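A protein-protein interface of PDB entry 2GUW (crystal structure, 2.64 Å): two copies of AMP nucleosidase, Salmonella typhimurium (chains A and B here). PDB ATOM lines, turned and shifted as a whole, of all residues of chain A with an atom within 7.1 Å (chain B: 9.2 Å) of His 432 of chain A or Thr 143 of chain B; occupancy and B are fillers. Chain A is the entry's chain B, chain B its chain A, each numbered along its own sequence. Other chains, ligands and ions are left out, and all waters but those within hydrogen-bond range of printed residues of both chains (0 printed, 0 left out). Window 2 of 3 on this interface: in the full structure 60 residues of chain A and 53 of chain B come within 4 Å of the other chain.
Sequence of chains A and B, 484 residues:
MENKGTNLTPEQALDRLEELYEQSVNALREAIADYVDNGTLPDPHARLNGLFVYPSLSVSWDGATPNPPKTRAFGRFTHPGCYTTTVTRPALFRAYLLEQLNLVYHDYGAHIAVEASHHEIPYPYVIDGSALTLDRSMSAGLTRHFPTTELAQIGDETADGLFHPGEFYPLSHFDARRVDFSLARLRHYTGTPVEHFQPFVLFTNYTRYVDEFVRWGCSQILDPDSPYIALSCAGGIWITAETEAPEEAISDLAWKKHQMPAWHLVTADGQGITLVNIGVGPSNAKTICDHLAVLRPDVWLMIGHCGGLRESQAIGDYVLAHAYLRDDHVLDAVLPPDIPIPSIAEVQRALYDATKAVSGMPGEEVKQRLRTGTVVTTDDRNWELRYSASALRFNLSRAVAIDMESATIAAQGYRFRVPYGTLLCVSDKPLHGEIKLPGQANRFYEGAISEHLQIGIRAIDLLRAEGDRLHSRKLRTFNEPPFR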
ATOM      1  N   GLY A 308      17.148  -5.712  18.885  1.00  0.00           N
ATOM      2  CA  GLY A 308      16.031  -4.811  19.080  1.00  0.00           C
ATOM      3  C   GLY A 308      14.801  -5.653  19.345  1.00  0.00           C
ATOM      4  O   GLY A 308      14.561  -6.637  18.641  1.00  0.00           O
ATOM      5  N   LEU A 309      14.024  -5.269  20.355  1.00  0.00           N
ATOM      6  CA  LEU A 309      12.829  -6.020  20.732  1.00  0.00           C
ATOM      7  C   LEU A 309      11.484  -5.394  20.360  1.00  0.00           C
ATOM      8  O   LEU A 309      10.445  -5.874  20.809  1.00  0.00           O
ATOM      9  CB  LEU A 309      12.857  -6.299  22.238  1.00  0.00           C
ATOM     10  CG  LEU A 309      14.043  -7.136  22.732  1.00  0.00           C
ATOM     11  CD1 LEU A 309      14.219  -6.914  24.213  1.00  0.00           C
ATOM     12  CD2 LEU A 309      13.828  -8.605  22.404  1.00  0.00           C
ATOM     13  N   ARG A 310      11.488  -4.335  19.554  1.00  0.00           N
ATOM     14  CA  ARG A 310      10.233  -3.689  19.149  1.00  0.00           C
ATOM     15  C   ARG A 310       9.940  -3.827  17.654  1.00  0.00           C
ATOM     16  O   ARG A 310      10.816  -3.634  16.805  1.00  0.00           O
ATOM     17  CB  ARG A 310      10.234  -2.203  19.526  1.00  0.00           C
ATOM     18  CG  ARG A 310      10.345  -1.916  21.021  1.00  0.00           C
ATOM     19  CD  ARG A 310       9.297  -2.651  21.834  1.00  0.00           C
ATOM     20  NE  ARG A 310       9.390  -2.328  23.257  1.00  0.00           N
ATOM     21  CZ  ARG A 310       9.091  -1.141  23.780  1.00  0.00           C
ATOM     22  NH1 ARG A 310       8.676  -0.157  22.997  1.00  0.00           N
ATOM     23  NH2 ARG A 310       9.203  -0.930  25.085  1.00  0.00           N
ATOM     24  N   GLU A 311       8.695  -4.166  17.345  1.00  0.00           N
ATOM     25  CA  GLU A 311       8.250  -4.337  15.963  1.00  0.00           C
ATOM     26  C   GLU A 311       8.739  -3.198  15.058  1.00  0.00           C
ATOM     27  O   GLU A 311       9.289  -3.447  13.992  1.00  0.00           O
ATOM     28  CB  GLU A 311       6.710  -4.434  15.929  1.00  0.00           C
ATOM     29  CG  GLU A 311       6.067  -4.494  14.538  1.00  0.00           C
ATOM     30  CD  GLU A 311       6.357  -5.793  13.788  1.00  0.00           C
ATOM     31  OE1 GLU A 311       7.545  -6.074  13.492  1.00  0.00           O
ATOM     32  OE2 GLU A 311       5.394  -6.535  13.490  1.00  0.00           O
ATOM     33  N   SER A 312       8.565  -1.957  15.501  1.00  0.00           N
ATOM     34  CA  SER A 312       8.965  -0.796  14.711  1.00  0.00           C
ATOM     35  C   SER A 312      10.467  -0.516  14.561  1.00  0.00           C
ATOM     36  O   SER A 312      10.853   0.412  13.849  1.00  0.00           O
ATOM     37  CB  SER A 312       8.307   0.457  15.272  1.00  0.00           C
ATOM     38  OG  SER A 312       8.861   0.770  16.533  1.00  0.00           O
ATOM     39  N   GLN A 313      11.323  -1.282  15.228  1.00  0.00           N
ATOM     40  CA  GLN A 313      12.754  -1.038  15.097  1.00  0.00           C
ATOM     41  C   GLN A 313      13.289  -1.594  13.783  1.00  0.00           C
ATOM     42  O   GLN A 313      12.791  -2.592  13.271  1.00  0.00           O
ATOM     43  CB  GLN A 313      13.514  -1.678  16.255  1.00  0.00           C
ATOM     44  CG  GLN A 313      13.251  -1.025  17.586  1.00  0.00           C
ATOM     45  CD  GLN A 313      14.059  -1.661  18.692  1.00  0.00           C
ATOM     46  OE1 GLN A 313      13.935  -2.860  18.937  1.00  0.00           O
ATOM     47  NE2 GLN A 313      14.900  -0.865  19.363  1.00  0.00           N
ATOM     48  N   LYS A 429      16.512  -8.669  14.756  1.00  0.00           N
ATOM     49  CA  LYS A 429      15.222  -8.602  15.426  1.00  0.00           C
ATOM     50  C   LYS A 429      14.758 -10.022  15.759  1.00  0.00           C
ATOM     51  O   LYS A 429      13.927 -10.594  15.048  1.00  0.00           O
ATOM     52  CB  LYS A 429      14.195  -7.930  14.512  1.00  0.00           C
ATOM     53  CG  LYS A 429      14.578  -6.545  14.032  1.00  0.00           C
ATOM     54  CD  LYS A 429      14.478  -5.540  15.149  1.00  0.00           C
ATOM     55  CE  LYS A 429      13.051  -5.447  15.693  1.00  0.00           C
ATOM     56  NZ  LYS A 429      12.060  -4.870  14.741  1.00  0.00           N
ATOM     57  N   PRO A 430      15.292 -10.603  16.846  1.00  0.00           N
ATOM     58  CA  PRO A 430      15.015 -11.948  17.364  1.00  0.00           C
ATOM     59  C   PRO A 430      13.538 -12.310  17.460  1.00  0.00           C
ATOM     60  O   PRO A 430      13.140 -13.427  17.157  1.00  0.00           O
ATOM     61  CB  PRO A 430      15.664 -11.924  18.735  1.00  0.00           C
ATOM     62  CG  PRO A 430      16.801 -10.973  18.537  1.00  0.00           C
ATOM     63  CD  PRO A 430      16.171  -9.865  17.767  1.00  0.00           C
ATOM     64  N   LEU A 431      12.718 -11.364  17.880  1.00  0.00           N
ATOM     65  CA  LEU A 431      11.300 -11.636  18.029  1.00  0.00           C
ATOM     66  C   LEU A 431      10.445 -11.401  16.793  1.00  0.00           C
ATOM     67  O   LEU A 431       9.253 -11.655  16.821  1.00  0.00           O
ATOM     68  CB  LEU A 431      10.741 -10.808  19.190  1.00  0.00           C
ATOM     69  CG  LEU A 431      10.792 -11.439  20.583  1.00  0.00           C
ATOM     70  CD1 LEU A 431      12.116 -12.135  20.828  1.00  0.00           C
ATOM     71  CD2 LEU A 431      10.536 -10.351  21.605  1.00  0.00           C
ATOM     72  N   HIS A 432      11.038 -10.931  15.704  1.00  0.00           N
ATOM     73  CA  HIS A 432      10.248 -10.657  14.515  1.00  0.00           C
ATOM     74  C   HIS A 432      10.695 -11.272  13.199  1.00  0.00           C
ATOM     75  O   HIS A 432      10.419 -10.710  12.136  1.00  0.00           O
ATOM     76  CB  HIS A 432      10.081  -9.147  14.350  1.00  0.00           C
ATOM     77  CG  HIS A 432       9.420  -8.500  15.523  1.00  0.00           C
ATOM     78  ND1 HIS A 432      10.117  -8.107  16.646  1.00  0.00           N
ATOM     79  CD2 HIS A 432       8.114  -8.255  15.787  1.00  0.00           C
ATOM     80  CE1 HIS A 432       9.268  -7.650  17.550  1.00  0.00           C
ATOM     81  NE2 HIS A 432       8.047  -7.729  17.054  1.00  0.00           N
ATOM     82  N   GLY A 433      11.383 -12.411  13.265  1.00  0.00           N
ATOM     83  CA  GLY A 433      11.795 -13.092  12.048  1.00  0.00           C
ATOM     84  C   GLY A 433      13.163 -12.819  11.454  1.00  0.00           C
ATOM     85  O   GLY A 433      13.439 -13.226  10.322  1.00  0.00           O
ATOM     86  N   GLU A 434      14.023 -12.133  12.198  1.00  0.00           N
ATOM     87  CA  GLU A 434      15.362 -11.839  11.710  1.00  0.00           C
ATOM     88  C   GLU A 434      16.418 -12.112  12.769  1.00  0.00           C
ATOM     89  O   GLU A 434      16.859 -11.203  13.475  1.00  0.00           O
ATOM     90  CB  GLU A 434      15.450 -10.390  11.244  1.00  0.00           C
ATOM     91  CG  GLU A 434      14.671 -10.120   9.979  1.00  0.00           C
ATOM     92  CD  GLU A 434      14.374  -8.649   9.787  1.00  0.00           C
ATOM     93  OE1 GLU A 434      13.597  -8.095  10.594  1.00  0.00           O
ATOM     94  OE2 GLU A 434      14.918  -8.049   8.835  1.00  0.00           O
ATOM     95  N   ILE A 435      16.803 -13.380  12.887  1.00  0.00           N
ATOM     96  CA  ILE A 435      17.829 -13.786  13.837  1.00  0.00           C
ATOM     97  C   ILE A 435      19.128 -13.831  13.050  1.00  0.00           C
ATOM     98  O   ILE A 435      19.172 -14.391  11.953  1.00  0.00           O
ATOM     99  CB  ILE A 435      17.553 -15.192  14.423  1.00  0.00           C
ATOM    100  CG1 ILE A 435      17.150 -16.151  13.291  1.00  0.00           C
ATOM    101  CG2 ILE A 435      16.497 -15.105  15.516  1.00  0.00           C
ATOM    102  CD1 ILE A 435      17.068 -17.626  13.698  1.00  0.00           C
ATOM    103  N   ILE B  32      10.974 -18.598  -3.162  1.00  0.00           N
ATOM    104  CA  ILE B  32      11.605 -17.356  -2.725  1.00  0.00           C
ATOM    105  C   ILE B  32      12.264 -16.624  -3.892  1.00  0.00           C
ATOM    106  O   ILE B  32      12.137 -15.403  -4.015  1.00  0.00           O
ATOM    107  CB  ILE B  32      12.651 -17.641  -1.622  1.00  0.00           C
ATOM    108  CG1 ILE B  32      11.936 -18.142  -0.364  1.00  0.00           C
ATOM    109  CG2 ILE B  32      13.464 -16.391  -1.325  1.00  0.00           C
ATOM    110  CD1 ILE B  32      12.866 -18.690   0.684  1.00  0.00           C
ATOM    111  N   TYR B  35       9.964 -14.921  -5.802  1.00  0.00           N
ATOM    112  CA  TYR B  35       9.445 -13.719  -5.161  1.00  0.00           C
ATOM    113  C   TYR B  35      10.383 -12.522  -5.277  1.00  0.00           C
ATOM    114  O   TYR B  35       9.932 -11.388  -5.439  1.00  0.00           O
ATOM    115  CB  TYR B  35       9.148 -14.001  -3.689  1.00  0.00           C
ATOM    116  CG  TYR B  35       8.397 -12.889  -2.993  1.00  0.00           C
ATOM    117  CD1 TYR B  35       9.060 -11.753  -2.526  1.00  0.00           C
ATOM    118  CD2 TYR B  35       7.017 -12.966  -2.817  1.00  0.00           C
ATOM    119  CE1 TYR B  35       8.368 -10.721  -1.900  1.00  0.00           C
ATOM    120  CE2 TYR B  35       6.313 -11.943  -2.195  1.00  0.00           C
ATOM    121  CZ  TYR B  35       6.993 -10.825  -1.740  1.00  0.00           C
ATOM    122  OH  TYR B  35       6.294  -9.815  -1.130  1.00  0.00           O
ATOM    123  N   ARG B  47       0.827 -25.134  -0.297  1.00  0.00           N
ATOM    124  CA  ARG B  47       1.558 -24.827   0.919  1.00  0.00           C
ATOM    125  C   ARG B  47       0.830 -25.491   2.086  1.00  0.00           C
ATOM    126  O   ARG B  47       1.439 -26.185   2.899  1.00  0.00           O
ATOM    127  CB  ARG B  47       1.613 -23.311   1.122  1.00  0.00           C
ATOM    128  CG  ARG B  47       2.688 -22.849   2.086  1.00  0.00           C
ATOM    129  CD  ARG B  47       2.626 -21.349   2.303  1.00  0.00           C
ATOM    130  NE  ARG B  47       3.609 -20.909   3.288  1.00  0.00           N
ATOM    131  CZ  ARG B  47       3.576 -19.728   3.897  1.00  0.00           C
ATOM    132  NH1 ARG B  47       2.606 -18.865   3.622  1.00  0.00           N
ATOM    133  NH2 ARG B  47       4.507 -19.409   4.787  1.00  0.00           N
ATOM    134  N   TYR B 123      12.925 -20.003   6.057  1.00  0.00           N
ATOM    135  CA  TYR B 123      13.774 -19.749   4.891  1.00  0.00           C
ATOM    136  C   TYR B 123      15.250 -19.441   5.172  1.00  0.00           C
ATOM    137  O   TYR B 123      16.129 -19.843   4.405  1.00  0.00           O
ATOM    138  CB  TYR B 123      13.148 -18.657   3.999  1.00  0.00           C
ATOM    139  CG  TYR B 123      13.351 -17.230   4.437  1.00  0.00           C
ATOM    140  CD1 TYR B 123      14.580 -16.591   4.258  1.00  0.00           C
ATOM    141  CD2 TYR B 123      12.318 -16.519   5.042  1.00  0.00           C
ATOM    142  CE1 TYR B 123      14.779 -15.273   4.672  1.00  0.00           C
ATOM    143  CE2 TYR B 123      12.498 -15.200   5.465  1.00  0.00           C
ATOM    144  CZ  TYR B 123      13.734 -14.582   5.279  1.00  0.00           C
ATOM    145  OH  TYR B 123      13.924 -13.284   5.719  1.00  0.00           O
ATOM    146  N   PRO B 124      15.551 -18.740   6.278  1.00  0.00           N
ATOM    147  CA  PRO B 124      16.962 -18.451   6.540  1.00  0.00           C
ATOM    148  C   PRO B 124      17.848 -19.693   6.563  1.00  0.00           C
ATOM    149  O   PRO B 124      19.063 -19.582   6.415  1.00  0.00           O
ATOM    150  CB  PRO B 124      16.918 -17.746   7.888  1.00  0.00           C
ATOM    151  CG  PRO B 124      15.622 -17.006   7.817  1.00  0.00           C
ATOM    152  CD  PRO B 124      14.694 -18.064   7.270  1.00  0.00           C
ATOM    153  N   LEU B 134      18.676  -7.863  -0.117  1.00  0.00           N
ATOM    154  CA  LEU B 134      17.707  -7.120  -0.893  1.00  0.00           C
ATOM    155  C   LEU B 134      17.576  -5.796  -0.165  1.00  0.00           C
ATOM    156  O   LEU B 134      18.395  -5.474   0.692  1.00  0.00           O
ATOM    157  CB  LEU B 134      16.358  -7.837  -0.876  1.00  0.00           C
ATOM    158  CG  LEU B 134      16.375  -9.368  -0.962  1.00  0.00           C
ATOM    159  CD1 LEU B 134      16.897  -9.957   0.344  1.00  0.00           C
ATOM    160  CD2 LEU B 134      14.963  -9.876  -1.232  1.00  0.00           C
ATOM    161  N   ARG B 136      15.139  -3.001   2.126  1.00  0.00           N
ATOM    162  CA  ARG B 136      14.249  -3.110   3.270  1.00  0.00           C
ATOM    163  C   ARG B 136      12.826  -3.555   2.944  1.00  0.00           C
ATOM    164  O   ARG B 136      12.229  -4.329   3.698  1.00  0.00           O
ATOM    165  CB  ARG B 136      14.225  -1.781   4.020  1.00  0.00           C
ATOM    166  CG  ARG B 136      15.554  -1.438   4.660  1.00  0.00           C
ATOM    167  CD  ARG B 136      15.524  -0.058   5.262  1.00  0.00           C
ATOM    168  NE  ARG B 136      16.795   0.266   5.894  1.00  0.00           N
ATOM    169  CZ  ARG B 136      17.233  -0.287   7.019  1.00  0.00           C
ATOM    170  NH1 ARG B 136      16.496  -1.197   7.642  1.00  0.00           N
ATOM    171  NH2 ARG B 136      18.410   0.071   7.518  1.00  0.00           N
ATOM    172  N   SER B 137      12.278  -3.072   1.833  1.00  0.00           N
ATOM    173  CA  SER B 137      10.921  -3.453   1.438  1.00  0.00           C
ATOM    174  C   SER B 137      10.840  -4.930   1.026  1.00  0.00           C
ATOM    175  O   SER B 137       9.888  -5.634   1.382  1.00  0.00           O
ATOM    176  CB  SER B 137      10.428  -2.567   0.288  1.00  0.00           C
ATOM    177  OG  SER B 137      10.216  -1.238   0.726  1.00  0.00           O
ATOM    178  N   MET B 138      11.836  -5.395   0.276  1.00  0.00           N
ATOM    179  CA  MET B 138      11.856  -6.785  -0.153  1.00  0.00           C
ATOM    180  C   MET B 138      11.987  -7.721   1.039  1.00  0.00           C
ATOM    181  O   MET B 138      11.280  -8.721   1.130  1.00  0.00           O
ATOM    182  CB  MET B 138      13.003  -7.032  -1.139  1.00  0.00           C
ATOM    183  CG  MET B 138      12.737  -6.509  -2.546  1.00  0.00           C
ATOM    184  SD  MET B 138      11.177  -7.139  -3.255  1.00  0.00           S
ATOM    185  CE  MET B 138      10.036  -5.747  -2.888  1.00  0.00           C
ATOM    186  N   SER B 139      12.889  -7.386   1.957  1.00  0.00           N
ATOM    187  CA  SER B 139      13.114  -8.211   3.142  1.00  0.00           C
ATOM    188  C   SER B 139      11.892  -8.277   4.055  1.00  0.00           C
ATOM    189  O   SER B 139      11.627  -9.304   4.678  1.00  0.00           O
ATOM    190  CB  SER B 139      14.333  -7.701   3.925  1.00  0.00           C
ATOM    191  OG  SER B 139      14.250  -6.305   4.161  1.00  0.00           O
ATOM    192  N   ALA B 140      11.147  -7.186   4.135  1.00  0.00           N
ATOM    193  CA  ALA B 140       9.953  -7.167   4.967  1.00  0.00           C
ATOM    194  C   ALA B 140       8.901  -8.073   4.338  1.00  0.00           C
ATOM    195  O   ALA B 140       8.037  -8.618   5.024  1.00  0.00           O
ATOM    196  CB  ALA B 140       9.422  -5.749   5.084  1.00  0.00           C
ATOM    197  N   GLY B 141       8.986  -8.226   3.021  1.00  0.00           N
ATOM    198  CA  GLY B 141       8.045  -9.068   2.309  1.00  0.00           C
ATOM    199  C   GLY B 141       8.336 -10.530   2.568  1.00  0.00           C
ATOM    200  O   GLY B 141       7.423 -11.354   2.623  1.00  0.00           O
ATOM    201  N   LEU B 142       9.616 -10.857   2.712  1.00  0.00           N
ATOM    202  CA  LEU B 142      10.011 -12.230   2.988  1.00  0.00           C
ATOM    203  C   LEU B 142       9.390 -12.585   4.330  1.00  0.00           C
ATOM    204  O   LEU B 142       8.832 -13.665   4.505  1.00  0.00           O
ATOM    205  CB  LEU B 142      11.539 -12.350   3.070  1.00  0.00           C
ATOM    206  CG  LEU B 142      12.328 -12.084   1.784  1.00  0.00           C
ATOM    207  CD1 LEU B 142      13.819 -12.098   2.076  1.00  0.00           C
ATOM    208  CD2 LEU B 142      11.976 -13.138   0.745  1.00  0.00           C
ATOM    209  N   THR B 143       9.478 -11.642   5.263  1.00  0.00           N
ATOM    210  CA  THR B 143       8.940 -11.809   6.604  1.00  0.00           C
ATOM    211  C   THR B 143       7.420 -11.929   6.621  1.00  0.00           C
ATOM    212  O   THR B 143       6.875 -12.879   7.184  1.00  0.00           O
ATOM    213  CB  THR B 143       9.353 -10.619   7.512  1.00  0.00           C
ATOM    214  OG1 THR B 143      10.719 -10.777   7.914  1.00  0.00           O
ATOM    215  CG2 THR B 143       8.460 -10.534   8.742  1.00  0.00           C
ATOM    216  N   ARG B 144       6.739 -10.974   5.993  1.00  0.00           N
ATOM    217  CA  ARG B 144       5.278 -10.966   5.978  1.00  0.00           C
ATOM    218  C   ARG B 144       4.634 -11.978   5.038  1.00  0.00           C
ATOM    219  O   ARG B 144       3.414 -11.982   4.886  1.00  0.00           O
ATOM    220  CB  ARG B 144       4.749  -9.561   5.637  1.00  0.00           C
ATOM    221  CG  ARG B 144       3.319  -9.313   6.138  1.00  0.00           C
ATOM    222  CD  ARG B 144       2.700  -8.004   5.647  1.00  0.00           C
ATOM    223  NE  ARG B 144       2.373  -8.052   4.223  1.00  0.00           N
ATOM    224  CZ  ARG B 144       1.484  -7.258   3.627  1.00  0.00           C
ATOM    225  NH1 ARG B 144       0.823  -6.349   4.333  1.00  0.00           N
ATOM    226  NH2 ARG B 144       1.255  -7.374   2.323  1.00  0.00           N
ATOM    227  N   HIS B 145       5.430 -12.842   4.417  1.00  0.00           N
ATOM    228  CA  HIS B 145       4.860 -13.816   3.492  1.00  0.00           C
ATOM    229  C   HIS B 145       5.397 -15.231   3.587  1.00  0.00           C
ATOM    230  O   HIS B 145       4.652 -16.190   3.393  1.00  0.00           O
ATOM    231  CB  HIS B 145       4.986 -13.297   2.058  1.00  0.00           C
ATOM    232  CG  HIS B 145       4.043 -12.176   1.753  1.00  0.00           C
ATOM    233  ND1 HIS B 145       2.674 -12.342   1.744  1.00  0.00           N
ATOM    234  CD2 HIS B 145       4.263 -10.860   1.525  1.00  0.00           C
ATOM    235  CE1 HIS B 145       2.092 -11.177   1.525  1.00  0.00           C
ATOM    236  NE2 HIS B 145       3.034 -10.260   1.391  1.00  0.00           N
ATOM    237  N   PHE B 146       6.680 -15.371   3.882  1.00  0.00           N
ATOM    238  CA  PHE B 146       7.259 -16.697   3.997  1.00  0.00           C
ATOM    239  C   PHE B 146       7.442 -17.108   5.451  1.00  0.00           C
ATOM    240  O   PHE B 146       7.216 -16.316   6.370  1.00  0.00           O
ATOM    241  CB  PHE B 146       8.596 -16.758   3.264  1.00  0.00           C
ATOM    242  CG  PHE B 146       8.479 -16.546   1.786  1.00  0.00           C
ATOM    243  CD1 PHE B 146       8.354 -15.265   1.261  1.00  0.00           C
ATOM    244  CD2 PHE B 146       8.457 -17.633   0.919  1.00  0.00           C
ATOM    245  CE1 PHE B 146       8.210 -15.069  -0.104  1.00  0.00           C
ATOM    246  CE2 PHE B 146       8.312 -17.447  -0.448  1.00  0.00           C
ATOM    247  CZ  PHE B 146       8.188 -16.162  -0.962  1.00  0.00           C
ATOM    248  N   PRO B 147       7.829 -18.371   5.680  1.00  0.00           N
ATOM    249  CA  PRO B 147       8.040 -18.870   7.041  1.00  0.00           C
ATOM    250  C   PRO B 147       9.385 -18.430   7.623  1.00  0.00           C
ATOM    251  O   PRO B 147      10.438 -18.620   7.003  1.00  0.00           O
ATOM    252  CB  PRO B 147       7.944 -20.384   6.862  1.00  0.00           C
ATOM    253  CG  PRO B 147       8.519 -20.589   5.495  1.00  0.00           C
ATOM    254  CD  PRO B 147       7.853 -19.481   4.707  1.00  0.00           C
ATOM    255  N   THR B 148       9.339 -17.832   8.811  1.00  0.00           N
ATOM    256  CA  THR B 148      10.549 -17.373   9.487  1.00  0.00           C
ATOM    257  C   THR B 148      10.700 -18.094  10.815  1.00  0.00           C
ATOM    258  O   THR B 148       9.943 -19.019  11.120  1.00  0.00           O
ATOM    259  CB  THR B 148      10.512 -15.860   9.775  1.00  0.00           C
ATOM    260  OG1 THR B 148       9.402 -15.564  10.631  1.00  0.00           O
ATOM    261  CG2 THR B 148      10.388 -15.069   8.483  1.00  0.00           C
ATOM    262  N   THR B 149      11.674 -17.658  11.606  1.00  0.00           N
ATOM    263  CA  THR B 149      11.928 -18.263  12.904  1.00  0.00           C
ATOM    264  C   THR B 149      10.821 -17.898  13.888  1.00  0.00           C
ATOM    265  O   THR B 149      10.337 -16.764  13.898  1.00  0.00           O
ATOM    266  CB  THR B 149      13.269 -17.789  13.484  1.00  0.00           C
ATOM    267  OG1 THR B 149      14.281 -17.852  12.470  1.00  0.00           O
ATOM    268  CG2 THR B 149      13.677 -18.678  14.650  1.00  0.00           C
ATOM    269  N   GLU B 150      10.425 -18.866  14.711  1.00  0.00           N
ATOM    270  CA  GLU B 150       9.374 -18.659  15.707  1.00  0.00           C
ATOM    271  C   GLU B 150       9.829 -19.165  17.083  1.00  0.00           C
ATOM    272  O   GLU B 150       9.806 -20.373  17.353  1.00  0.00           O
ATOM    273  CB  GLU B 150       8.086 -19.388  15.281  1.00  0.00           C
ATOM    274  CG  GLU B 150       6.836 -18.496  15.184  1.00  0.00           C
ATOM    275  CD  GLU B 150       6.301 -18.045  16.542  1.00  0.00           C
ATOM    276  OE1 GLU B 150       7.021 -17.325  17.275  1.00  0.00           O
ATOM    277  OE2 GLU B 150       5.150 -18.412  16.872  1.00  0.00           O
ATOM    278  N   LEU B 151      10.238 -18.233  17.944  1.00  0.00           N
ATOM    279  CA  LEU B 151      10.703 -18.567  19.291  1.00  0.00           C
ATOM    280  C   LEU B 151       9.620 -19.302  20.086  1.00  0.00           C
ATOM    281  O   LEU B 151       9.862 -20.390  20.616  1.00  0.00           O
ATOM    282  CB  LEU B 151      11.115 -17.297  20.047  1.00  0.00           C
ATOM    283  CG  LEU B 151      12.022 -16.300  19.323  1.00  0.00           C
ATOM    284  CD1 LEU B 151      13.188 -17.031  18.671  1.00  0.00           C
ATOM    285  CD2 LEU B 151      11.210 -15.560  18.274  1.00  0.00           C
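Of chain B, only Thr 148 (3.7 Å) comes within 4 Å of Gly 433 of chain A. Of the printed residues of chain A, Leu 151 of chain B touches Pro 430 and Leu 431. Printed residues of chain A within 4 Å of Thr 148 of chain B: Gly 433. Of the printed residues of chain B, Pro 430 of chain A touches Leu 151 (3.1 Å). The nearest residue of chain A that does not touch Thr 143 of chain B is Gly 433 of chain A (4.4 Å). The nearest printed residue of chain B that does not touch Ile 435 of chain A is Leu 151 of chain B (5.0 Å).
Among the printed residues, merely in contact across the chains: Pro 430 of chain A with Leu 151 of chain B (3.1 Å), Leu 431 of chain A with Leu 151 of chain B (3.9 Å), His 432 of chain A with Thr 143 of chain B (3.9 Å), Gly 433 of chain A with Thr 148 of chain B (3.7 Å) and Ile 435 of chain A with Thr 149 of chain B (3.1 Å).
No position is printed for both chains.
Of the 22 printed residues of chain B, 4 touch a printed residue of chain A. Of the 13 printed residues of chain A, 5 touch a printed residue of chain B. Among the printed residues, 5 pairs touch across the chains. Among the printed residues, no Asp or Glu carboxylate lies within 4 Å of a Lys or Arg side-chain nitrogen of the other chain.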
